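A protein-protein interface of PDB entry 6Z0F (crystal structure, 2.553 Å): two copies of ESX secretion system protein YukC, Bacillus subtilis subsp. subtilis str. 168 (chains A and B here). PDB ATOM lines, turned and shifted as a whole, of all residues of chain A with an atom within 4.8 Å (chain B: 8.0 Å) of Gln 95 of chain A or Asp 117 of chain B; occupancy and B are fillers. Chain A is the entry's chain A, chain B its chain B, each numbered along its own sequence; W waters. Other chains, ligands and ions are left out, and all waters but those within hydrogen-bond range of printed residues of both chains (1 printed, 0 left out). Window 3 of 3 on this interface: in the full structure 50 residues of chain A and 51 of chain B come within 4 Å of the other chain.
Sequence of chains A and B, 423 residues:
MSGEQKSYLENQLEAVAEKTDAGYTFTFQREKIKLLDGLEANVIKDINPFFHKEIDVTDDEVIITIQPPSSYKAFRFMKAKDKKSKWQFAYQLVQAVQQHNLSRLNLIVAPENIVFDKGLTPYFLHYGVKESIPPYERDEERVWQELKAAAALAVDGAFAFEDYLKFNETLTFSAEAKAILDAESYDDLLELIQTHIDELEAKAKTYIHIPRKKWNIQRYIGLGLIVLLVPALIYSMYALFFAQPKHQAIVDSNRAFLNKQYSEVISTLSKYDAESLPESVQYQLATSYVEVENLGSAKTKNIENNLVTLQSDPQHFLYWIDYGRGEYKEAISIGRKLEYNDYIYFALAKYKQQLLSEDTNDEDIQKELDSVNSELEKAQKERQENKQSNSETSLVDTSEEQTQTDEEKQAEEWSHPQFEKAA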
ATOM      1  N   TYR A  91      12.736  24.141 -21.947  1.00  0.00           N
ATOM      2  CA  TYR A  91      11.542  24.320 -22.780  1.00  0.00           C
ATOM      3  C   TYR A  91      11.109  25.772 -22.771  1.00  0.00           C
ATOM      4  O   TYR A  91      10.742  26.316 -23.811  1.00  0.00           O
ATOM      5  CB  TYR A  91      10.377  23.433 -22.297  1.00  0.00           C
ATOM      6  CG  TYR A  91       9.222  23.360 -23.277  1.00  0.00           C
ATOM      7  CD1 TYR A  91       9.302  22.575 -24.418  1.00  0.00           C
ATOM      8  CD2 TYR A  91       8.038  24.044 -23.041  1.00  0.00           C
ATOM      9  CE1 TYR A  91       8.239  22.485 -25.308  1.00  0.00           C
ATOM     10  CE2 TYR A  91       6.972  23.974 -23.932  1.00  0.00           C
ATOM     11  CZ  TYR A  91       7.077  23.195 -25.070  1.00  0.00           C
ATOM     12  OH  TYR A  91       6.019  23.100 -25.956  1.00  0.00           O
ATOM     13  N   GLN A  92      11.150  26.403 -21.594  1.00  0.00           N
ATOM     14  CA  GLN A  92      10.754  27.789 -21.451  1.00  0.00           C
ATOM     15  C   GLN A  92      11.834  28.757 -21.979  1.00  0.00           C
ATOM     16  O   GLN A  92      11.500  29.877 -22.345  1.00  0.00           O
ATOM     17  CB  GLN A  92      10.411  28.090 -19.991  1.00  0.00           C
ATOM     18  CG  GLN A  92       9.124  27.424 -19.545  1.00  0.00           C
ATOM     19  CD  GLN A  92       8.701  27.946 -18.200  1.00  0.00           C
ATOM     20  OE1 GLN A  92       8.971  27.342 -17.164  1.00  0.00           O
ATOM     21  NE2 GLN A  92       8.036  29.084 -18.171  1.00  0.00           N
ATOM     22  N   LEU A  93      13.102  28.336 -22.032  1.00  0.00           N
ATOM     23  CA  LEU A  93      14.172  29.179 -22.547  1.00  0.00           C
ATOM     24  C   LEU A  93      14.036  29.289 -24.063  1.00  0.00           C
ATOM     25  O   LEU A  93      14.121  30.392 -24.594  1.00  0.00           O
ATOM     26  CB  LEU A  93      15.550  28.634 -22.140  1.00  0.00           C
ATOM     27  CG  LEU A  93      16.746  29.479 -22.552  1.00  0.00           C
ATOM     28  CD1 LEU A  93      16.682  30.866 -21.949  1.00  0.00           C
ATOM     29  CD2 LEU A  93      18.033  28.807 -22.166  1.00  0.00           C
ATOM     30  N   VAL A  94      13.763  28.164 -24.751  1.00  0.00           N
ATOM     31  CA  VAL A  94      13.538  28.150 -26.201  1.00  0.00           C
ATOM     32  C   VAL A  94      12.315  28.992 -26.544  1.00  0.00           C
ATOM     33  O   VAL A  94      12.340  29.761 -27.498  1.00  0.00           O
ATOM     34  CB  VAL A  94      13.362  26.711 -26.744  1.00  0.00           C
ATOM     35  CG1 VAL A  94      13.020  26.723 -28.232  1.00  0.00           C
ATOM     36  CG2 VAL A  94      14.608  25.873 -26.489  1.00  0.00           C
ATOM     37  N   GLN A  95      11.247  28.855 -25.752  1.00  0.00           N
ATOM     38  CA  GLN A  95      10.011  29.594 -25.965  1.00  0.00           C
ATOM     39  C   GLN A  95      10.214  31.088 -25.815  1.00  0.00           C
ATOM     40  O   GLN A  95       9.645  31.828 -26.589  1.00  0.00           O
ATOM     41  CB  GLN A  95       8.929  29.135 -24.983  1.00  0.00           C
ATOM     42  CG  GLN A  95       8.213  27.851 -25.368  1.00  0.00           C
ATOM     43  CD  GLN A  95       7.109  27.576 -24.373  1.00  0.00           C
ATOM     44  OE1 GLN A  95       7.304  27.644 -23.147  1.00  0.00           O
ATOM     45  NE2 GLN A  95       5.913  27.289 -24.872  1.00  0.00           N
ATOM     46  N   ALA A  96      11.012  31.541 -24.835  1.00  0.00           N
ATOM     47  CA  ALA A  96      11.256  32.972 -24.621  1.00  0.00           C
ATOM     48  C   ALA A  96      12.051  33.596 -25.768  1.00  0.00           C
ATOM     49  O   ALA A  96      11.884  34.779 -26.051  1.00  0.00           O
ATOM     50  CB  ALA A  96      11.984  33.194 -23.309  1.00  0.00           C
ATOM     51  N   VAL A  97      12.916  32.815 -26.421  1.00  0.00           N
ATOM     52  CA  VAL A  97      13.685  33.275 -27.568  1.00  0.00           C
ATOM     53  C   VAL A  97      12.776  33.296 -28.808  1.00  0.00           C
ATOM     54  O   VAL A  97      12.765  34.273 -29.557  1.00  0.00           O
ATOM     55  CB  VAL A  97      14.920  32.371 -27.768  1.00  0.00           C
ATOM     56  CG1 VAL A  97      15.623  32.684 -29.074  1.00  0.00           C
ATOM     57  CG2 VAL A  97      15.879  32.512 -26.601  1.00  0.00           C
ATOM     58  N   GLN A  98      11.981  32.236 -28.988  1.00  0.00           N
ATOM     59  CA  GLN A  98      11.039  32.071 -30.092  1.00  0.00           C
ATOM     60  C   GLN A  98       9.924  33.131 -30.043  1.00  0.00           C
ATOM     61  O   GLN A  98       9.479  33.604 -31.084  1.00  0.00           O
ATOM     62  CB  GLN A  98      10.424  30.669 -30.011  1.00  0.00           C
ATOM     63  CG  GLN A  98       9.819  30.158 -31.303  1.00  0.00           C
ATOM     64  CD  GLN A  98       8.948  28.940 -31.089  1.00  0.00           C
ATOM     65  OE1 GLN A  98       8.405  28.715 -29.997  1.00  0.00           O
ATOM     66  NE2 GLN A  98       8.777  28.134 -32.131  1.00  0.00           N
ATOM     67  N   GLN A  99       9.481  33.505 -28.843  1.00  0.00           N
ATOM     68  CA  GLN A  99       8.397  34.473 -28.660  1.00  0.00           C
ATOM     69  C   GLN A  99       8.871  35.941 -28.602  1.00  0.00           C
ATOM     70  O   GLN A  99       8.034  36.835 -28.454  1.00  0.00           O
ATOM     71  CB  GLN A  99       7.596  34.152 -27.388  1.00  0.00           C
ATOM     72  CG  GLN A  99       6.714  32.905 -27.506  1.00  0.00           C
ATOM     73  CD  GLN A  99       6.290  32.335 -26.164  1.00  0.00           C
ATOM     74  OE1 GLN A  99       6.668  32.826 -25.085  1.00  0.00           O
ATOM     75  NE2 GLN A  99       5.505  31.264 -26.209  1.00  0.00           N
ATOM     76  N   LEU A 190      11.902  21.974 -29.535  1.00  0.00           N
ATOM     77  CA  LEU A 190      10.777  21.965 -28.605  1.00  0.00           C
ATOM     78  C   LEU A 190      10.188  20.564 -28.492  1.00  0.00           C
ATOM     79  O   LEU A 190       9.783  20.176 -27.402  1.00  0.00           O
ATOM     80  CB  LEU A 190       9.685  22.962 -29.031  1.00  0.00           C
ATOM     81  CG  LEU A 190       9.985  24.431 -28.761  1.00  0.00           C
ATOM     82  CD1 LEU A 190       8.919  25.319 -29.346  1.00  0.00           C
ATOM     83  CD2 LEU A 190      10.139  24.695 -27.292  1.00  0.00           C
ATOM     84  N   PHE B  50       1.074  32.423 -31.962  1.00  0.00           N
ATOM     85  CA  PHE B  50       1.285  30.997 -32.195  1.00  0.00           C
ATOM     86  C   PHE B  50      -0.068  30.234 -32.199  1.00  0.00           C
ATOM     87  O   PHE B  50      -0.169  29.183 -32.831  1.00  0.00           O
ATOM     88  CB  PHE B  50       2.284  30.394 -31.174  1.00  0.00           C
ATOM     89  CG  PHE B  50       2.285  30.968 -29.769  1.00  0.00           C
ATOM     90  CD1 PHE B  50       2.802  32.229 -29.515  1.00  0.00           C
ATOM     91  CD2 PHE B  50       1.852  30.212 -28.693  1.00  0.00           C
ATOM     92  CE1 PHE B  50       2.805  32.750 -28.228  1.00  0.00           C
ATOM     93  CE2 PHE B  50       1.867  30.733 -27.403  1.00  0.00           C
ATOM     94  CZ  PHE B  50       2.337  31.999 -27.181  1.00  0.00           C
ATOM     95  N   PHE B  51      -1.111  30.784 -31.536  1.00  0.00           N
ATOM     96  CA  PHE B  51      -2.464  30.228 -31.533  1.00  0.00           C
ATOM     97  C   PHE B  51      -3.188  30.670 -32.797  1.00  0.00           C
ATOM     98  O   PHE B  51      -3.226  31.863 -33.093  1.00  0.00           O
ATOM     99  CB  PHE B  51      -3.266  30.714 -30.314  1.00  0.00           C
ATOM    100  CG  PHE B  51      -2.878  30.221 -28.941  1.00  0.00           C
ATOM    101  CD1 PHE B  51      -1.678  29.573 -28.733  1.00  0.00           C
ATOM    102  CD2 PHE B  51      -3.692  30.454 -27.852  1.00  0.00           C
ATOM    103  CE1 PHE B  51      -1.318  29.144 -27.467  1.00  0.00           C
ATOM    104  CE2 PHE B  51      -3.326  30.025 -26.589  1.00  0.00           C
ATOM    105  CZ  PHE B  51      -2.142  29.372 -26.405  1.00  0.00           C
ATOM    106  N   PRO B  69      -1.337  25.148 -29.914  1.00  0.00           N
ATOM    107  CA  PRO B  69      -0.593  23.964 -30.382  1.00  0.00           C
ATOM    108  C   PRO B  69      -1.088  22.669 -29.742  1.00  0.00           C
ATOM    109  O   PRO B  69      -1.529  22.682 -28.598  1.00  0.00           O
ATOM    110  CB  PRO B  69       0.849  24.271 -29.975  1.00  0.00           C
ATOM    111  CG  PRO B  69       0.908  25.749 -29.899  1.00  0.00           C
ATOM    112  CD  PRO B  69      -0.425  26.170 -29.367  1.00  0.00           C
ATOM    113  N   SER B  71       0.215  20.099 -28.360  1.00  0.00           N
ATOM    114  CA  SER B  71       0.841  19.753 -27.080  1.00  0.00           C
ATOM    115  C   SER B  71       0.243  20.489 -25.875  1.00  0.00           C
ATOM    116  O   SER B  71       0.456  20.057 -24.744  1.00  0.00           O
ATOM    117  CB  SER B  71       2.337  20.034 -27.136  1.00  0.00           C
ATOM    118  OG  SER B  71       2.607  21.338 -27.623  1.00  0.00           O
ATOM    119  N   TYR B  72      -0.489  21.589 -26.102  1.00  0.00           N
ATOM    120  CA  TYR B  72      -1.091  22.358 -25.011  1.00  0.00           C
ATOM    121  C   TYR B  72      -2.333  21.639 -24.514  1.00  0.00           C
ATOM    122  O   TYR B  72      -3.174  21.251 -25.319  1.00  0.00           O
ATOM    123  CB  TYR B  72      -1.433  23.791 -25.449  1.00  0.00           C
ATOM    124  CG  TYR B  72      -0.238  24.687 -25.699  1.00  0.00           C
ATOM    125  CD1 TYR B  72       0.930  24.186 -26.257  1.00  0.00           C
ATOM    126  CD2 TYR B  72      -0.301  26.047 -25.445  1.00  0.00           C
ATOM    127  CE1 TYR B  72       2.018  25.008 -26.515  1.00  0.00           C
ATOM    128  CE2 TYR B  72       0.772  26.883 -25.718  1.00  0.00           C
ATOM    129  CZ  TYR B  72       1.936  26.359 -26.242  1.00  0.00           C
ATOM    130  OH  TYR B  72       3.004  27.189 -26.496  1.00  0.00           O
ATOM    131  N   LYS B  73      -2.433  21.423 -23.202  1.00  0.00           N
ATOM    132  CA  LYS B  73      -3.556  20.695 -22.626  1.00  0.00           C
ATOM    133  C   LYS B  73      -4.492  21.605 -21.845  1.00  0.00           C
ATOM    134  O   LYS B  73      -4.061  22.616 -21.312  1.00  0.00           O
ATOM    135  CB  LYS B  73      -3.052  19.573 -21.706  1.00  0.00           C
ATOM    136  CG  LYS B  73      -2.102  18.613 -22.391  1.00  0.00           C
ATOM    137  CD  LYS B  73      -2.780  17.309 -22.717  1.00  0.00           C
ATOM    138  CE  LYS B  73      -1.937  16.463 -23.633  1.00  0.00           C
ATOM    139  NZ  LYS B  73      -1.816  17.088 -24.977  1.00  0.00           N
ATOM    140  N   ALA B  74      -5.768  21.209 -21.737  1.00  0.00           N
ATOM    141  CA  ALA B  74      -6.786  21.953 -21.000  1.00  0.00           C
ATOM    142  C   ALA B  74      -6.554  21.897 -19.478  1.00  0.00           C
ATOM    143  O   ALA B  74      -5.910  20.974 -18.983  1.00  0.00           O
ATOM    144  CB  ALA B  74      -8.160  21.399 -21.332  1.00  0.00           C
ATOM    145  N   MET B  78      -4.468  19.287 -15.074  1.00  0.00           N
ATOM    146  CA  MET B  78      -3.549  19.631 -13.995  1.00  0.00           C
ATOM    147  C   MET B  78      -3.787  18.726 -12.789  1.00  0.00           C
ATOM    148  O   MET B  78      -2.835  18.346 -12.117  1.00  0.00           O
ATOM    149  CB  MET B  78      -3.695  21.106 -13.573  1.00  0.00           C
ATOM    150  CG  MET B  78      -2.826  22.074 -14.354  1.00  0.00           C
ATOM    151  SD  MET B  78      -1.060  21.678 -14.456  1.00  0.00           S
ATOM    152  CE  MET B  78      -0.669  21.453 -12.767  1.00  0.00           C
ATOM    153  N   LYS B  81      -1.538  15.760 -12.063  1.00  0.00           N
ATOM    154  CA  LYS B  81      -0.108  16.005 -11.844  1.00  0.00           C
ATOM    155  C   LYS B  81       0.247  15.968 -10.332  1.00  0.00           C
ATOM    156  O   LYS B  81      -0.635  15.809  -9.489  1.00  0.00           O
ATOM    157  CB  LYS B  81       0.297  17.363 -12.461  1.00  0.00           C
ATOM    158  CG  LYS B  81       0.108  17.438 -13.957  1.00  0.00           C
ATOM    159  CD  LYS B  81       1.034  18.465 -14.559  1.00  0.00           C
ATOM    160  CE  LYS B  81       0.877  18.542 -16.050  1.00  0.00           C
ATOM    161  NZ  LYS B  81       1.120  17.232 -16.704  1.00  0.00           N
ATOM    162  N   PHE B  89       2.380  25.775 -11.516  1.00  0.00           N
ATOM    163  CA  PHE B  89       1.374  26.222 -12.463  1.00  0.00           C
ATOM    164  C   PHE B  89       0.642  27.426 -11.874  1.00  0.00           C
ATOM    165  O   PHE B  89       0.424  28.407 -12.575  1.00  0.00           O
ATOM    166  CB  PHE B  89       0.401  25.076 -12.778  1.00  0.00           C
ATOM    167  CG  PHE B  89      -0.857  25.486 -13.514  1.00  0.00           C
ATOM    168  CD1 PHE B  89      -0.836  25.721 -14.879  1.00  0.00           C
ATOM    169  CD2 PHE B  89      -2.064  25.613 -12.842  1.00  0.00           C
ATOM    170  CE1 PHE B  89      -1.997  26.076 -15.555  1.00  0.00           C
ATOM    171  CE2 PHE B  89      -3.218  25.979 -13.524  1.00  0.00           C
ATOM    172  CZ  PHE B  89      -3.176  26.203 -14.875  1.00  0.00           C
ATOM    173  N   GLN B  92       2.804  30.594 -12.075  1.00  0.00           N
ATOM    174  CA  GLN B  92       2.808  31.140 -13.418  1.00  0.00           C
ATOM    175  C   GLN B  92       1.427  31.663 -13.853  1.00  0.00           C
ATOM    176  O   GLN B  92       1.359  32.526 -14.726  1.00  0.00           O
ATOM    177  CB  GLN B  92       3.316  30.090 -14.399  1.00  0.00           C
ATOM    178  CG  GLN B  92       4.795  29.815 -14.232  1.00  0.00           C
ATOM    179  CD  GLN B  92       5.291  28.994 -15.377  1.00  0.00           C
ATOM    180  OE1 GLN B  92       5.898  29.509 -16.315  1.00  0.00           O
ATOM    181  NE2 GLN B  92       5.019  27.707 -15.330  1.00  0.00           N
ATOM    182  N   VAL B 115      -5.424  26.904 -20.916  1.00  0.00           N
ATOM    183  CA  VAL B 115      -4.649  25.782 -21.429  1.00  0.00           C
ATOM    184  C   VAL B 115      -3.217  25.953 -20.899  1.00  0.00           C
ATOM    185  O   VAL B 115      -2.860  27.036 -20.441  1.00  0.00           O
ATOM    186  CB  VAL B 115      -4.682  25.631 -22.971  1.00  0.00           C
ATOM    187  CG1 VAL B 115      -6.094  25.379 -23.479  1.00  0.00           C
ATOM    188  CG2 VAL B 115      -4.052  26.830 -23.665  1.00  0.00           C
ATOM    189  N   PHE B 116      -2.404  24.897 -20.923  1.00  0.00           N
ATOM    190  CA  PHE B 116      -1.020  24.993 -20.453  1.00  0.00           C
ATOM    191  C   PHE B 116      -0.091  24.146 -21.325  1.00  0.00           C
ATOM    192  O   PHE B 116      -0.528  23.173 -21.938  1.00  0.00           O
ATOM    193  CB  PHE B 116      -0.883  24.636 -18.960  1.00  0.00           C
ATOM    194  CG  PHE B 116      -1.210  23.214 -18.592  1.00  0.00           C
ATOM    195  CD1 PHE B 116      -2.504  22.845 -18.273  1.00  0.00           C
ATOM    196  CD2 PHE B 116      -0.221  22.258 -18.517  1.00  0.00           C
ATOM    197  CE1 PHE B 116      -2.805  21.535 -17.938  1.00  0.00           C
ATOM    198  CE2 PHE B 116      -0.529  20.948 -18.192  1.00  0.00           C
ATOM    199  CZ  PHE B 116      -1.817  20.597 -17.894  1.00  0.00           C
ATOM    200  N   ASP B 117       1.185  24.532 -21.408  1.00  0.00           N
ATOM    201  CA  ASP B 117       2.152  23.813 -22.233  1.00  0.00           C
ATOM    202  C   ASP B 117       3.021  22.843 -21.375  1.00  0.00           C
ATOM    203  O   ASP B 117       2.794  22.727 -20.166  1.00  0.00           O
ATOM    204  CB  ASP B 117       3.016  24.828 -23.012  1.00  0.00           C
ATOM    205  CG  ASP B 117       3.766  25.822 -22.147  1.00  0.00           C
ATOM    206  OD1 ASP B 117       3.813  25.622 -20.912  1.00  0.00           O
ATOM    207  OD2 ASP B 117       4.322  26.789 -22.707  1.00  0.00           O
ATOM    208  N   LYS B 118       4.024  22.177 -21.988  1.00  0.00           N
ATOM    209  CA  LYS B 118       4.918  21.236 -21.303  1.00  0.00           C
ATOM    210  C   LYS B 118       5.693  21.870 -20.131  1.00  0.00           C
ATOM    211  O   LYS B 118       6.064  21.163 -19.191  1.00  0.00           O
ATOM    212  CB  LYS B 118       5.899  20.615 -22.302  1.00  0.00           C
ATOM    213  CG  LYS B 118       5.191  19.808 -23.371  1.00  0.00           C
ATOM    214  CD  LYS B 118       4.573  18.559 -22.785  1.00  0.00           C
ATOM    215  CE  LYS B 118       3.244  18.237 -23.403  1.00  0.00           C
ATOM    216  NZ  LYS B 118       2.676  16.995 -22.819  1.00  0.00           N
ATOM    217  N   GLY B 119       5.914  23.182 -20.193  1.00  0.00           N
ATOM    218  CA  GLY B 119       6.597  23.917 -19.140  1.00  0.00           C
ATOM    219  C   GLY B 119       5.671  24.416 -18.049  1.00  0.00           C
ATOM    220  O   GLY B 119       6.094  25.210 -17.206  1.00  0.00           O
ATOM    221  N   LEU B 120       4.398  23.949 -18.053  1.00  0.00           N
ATOM    222  CA  LEU B 120       3.325  24.271 -17.105  1.00  0.00           C
ATOM    223  C   LEU B 120       2.894  25.736 -17.173  1.00  0.00           C
ATOM    224  O   LEU B 120       2.311  26.229 -16.211  1.00  0.00           O
ATOM    225  CB  LEU B 120       3.712  23.918 -15.653  1.00  0.00           C
ATOM    226  CG  LEU B 120       4.289  22.528 -15.413  1.00  0.00           C
ATOM    227  CD1 LEU B 120       4.707  22.362 -13.985  1.00  0.00           C
ATOM    228  CD2 LEU B 120       3.310  21.448 -15.818  1.00  0.00           C
ATOM    229  N   THR B 121       3.168  26.437 -18.285  1.00  0.00           N
ATOM    230  CA  THR B 121       2.793  27.840 -18.434  1.00  0.00           C
ATOM    231  C   THR B 121       1.342  27.937 -18.859  1.00  0.00           C
ATOM    232  O   THR B 121       0.958  27.292 -19.828  1.00  0.00           O
ATOM    233  CB  THR B 121       3.683  28.535 -19.472  1.00  0.00           C
ATOM    234  OG1 THR B 121       5.059  28.218 -19.256  1.00  0.00           O
ATOM    235  CG2 THR B 121       3.478  30.023 -19.504  1.00  0.00           C
ATOM    236  N   PRO B 122       0.519  28.751 -18.175  1.00  0.00           N
ATOM    237  CA  PRO B 122      -0.883  28.876 -18.580  1.00  0.00           C
ATOM    238  C   PRO B 122      -1.103  29.960 -19.642  1.00  0.00           C
ATOM    239  O   PRO B 122      -0.358  30.938 -19.730  1.00  0.00           O
ATOM    240  CB  PRO B 122      -1.586  29.227 -17.278  1.00  0.00           C
ATOM    241  CG  PRO B 122      -0.557  29.937 -16.485  1.00  0.00           C
ATOM    242  CD  PRO B 122       0.809  29.567 -16.987  1.00  0.00           C
ATOM    243  N   TYR B 123      -2.133  29.757 -20.467  1.00  0.00           N
ATOM    244  CA  TYR B 123      -2.531  30.651 -21.547  1.00  0.00           C
ATOM    245  C   TYR B 123      -4.040  30.792 -21.575  1.00  0.00           C
ATOM    246  O   TYR B 123      -4.750  29.810 -21.363  1.00  0.00           O
ATOM    247  CB  TYR B 123      -2.060  30.111 -22.900  1.00  0.00           C
ATOM    248  CG  TYR B 123      -0.567  29.941 -23.040  1.00  0.00           C
ATOM    249  CD1 TYR B 123       0.047  28.740 -22.723  1.00  0.00           C
ATOM    250  CD2 TYR B 123       0.218  30.951 -23.570  1.00  0.00           C
ATOM    251  CE1 TYR B 123       1.417  28.573 -22.856  1.00  0.00           C
ATOM    252  CE2 TYR B 123       1.587  30.788 -23.732  1.00  0.00           C
ATOM    253  CZ  TYR B 123       2.183  29.591 -23.381  1.00  0.00           C
ATOM    254  OH  TYR B 123       3.539  29.418 -23.543  1.00  0.00           O
HETATM  255  O   HOH W   1       8.118  25.417 -15.268  1.00  0.00           O
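Of the 10 printed residues of chain A, 4 touch a printed residue of chain B.
Hydrophobic or aromatic side chains of chain A within 4 Å of the printed part of chain B: Tyr 91.
Hydrophobic or aromatic side chains of chain B that line the printed part of chain A: Phe 50, Tyr 72 and Tyr 123.
Gln 92 of chain B touches its own counterpart, Gln 92 of chain A.
1 position is printed for both chains.
Water W1 lies within hydrogen-bond range of O of Gly 119 of chain B and OE1 of Gln 92 of chain A.
Among the printed residues, merely in contact across the chains: Gln 99 of chain A with Phe 50 of chain B, Gln 92 of chain A with Gly 119 of chain B, Tyr 91 of chain A with Gly 119 of chain B, Gln 99 of chain A with Tyr 123 of chain B and Tyr 91 of chain A with Lys 118 of chain B.
The backbone carbonyl oxygen of Gln 95 of chain A sits close to the side-chain amide oxygen of Gln 99 of chain A, at 3.5 Å.
The side-chain amide nitrogen of Gln 92 of chain B sits at hydrogen-bond distance from the backbone carbonyl oxygen of Leu 120 of chain B, 3.2 Å away.
The side-chain amide oxygen (OE1) of Gln 92 of chain B lies within hydrogen-bond range of the side-chain hydroxyl (OG1) of Thr 121 of chain B.
OD1 of Asp 117 of chain B lies close to N of Gly 119 of chain B, 3.3 Å away.
The backbone NH (N) of Thr 121 of chain B is in hydrogen-bond range of the side-chain carboxylate (OD1) of Asp 117 of chain B (2.8 Å).
OD2 of Asp 117 of chain B is in hydrogen-bond range of OH of Tyr 123 of chain B, at 2.9 Å.
Gln 95 of chain A touches just these residues of chain B: Tyr 72 (3.3 Å), Asp 117 (2.7 Å) and Tyr 123 (3.5 Å).
Of the printed residues of chain A, Asp 117 of chain B touches Gln 95.
No residue of chain B comes within 4 Å of Ala 96 of chain A.
Printed residues of chain B within 4 Å of Gln 92 of chain A: Gln 92 (2.9 Å), Gly 119 (3.6 Å) and Thr 121 (3.3 Å).
Printed residues of chain A within 4 Å of Phe 50 of chain B: Gln 99.
Of the printed residues of chain A, Tyr 72 of chain B touches Gln 95.
Val 94 of chain A touches none of the printed residues of chain B.
The nearest residue of chain A that does not touch Asp 117 of chain B is Tyr 91 of chain A (4.1 Å).
The nearest printed residue of chain A that does not touch Tyr 123 of chain B is Tyr 91 of chain A (6.4 Å).
The side-chain amide nitrogen of Gln 92 of chain A sits at hydrogen-bond distance from the side-chain amide oxygen of Gln 92 of chain B (2.9 Å).
OG1 of Thr 121 of chain B is in hydrogen-bond range of NE2 of Gln 92 of chain A, 3.3 Å away.
OH of Tyr 72 of chain B is in hydrogen-bond range of NE2 of Gln 95 of chain A.
NE2 of Gln 95 of chain A lies within hydrogen-bond range of OD2 of Asp 117 of chain B, at 2.7 Å.
OH of Tyr 123 of chain B sits at hydrogen-bond distance from NE2 of Gln 95 of chain A (3.5 Å).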
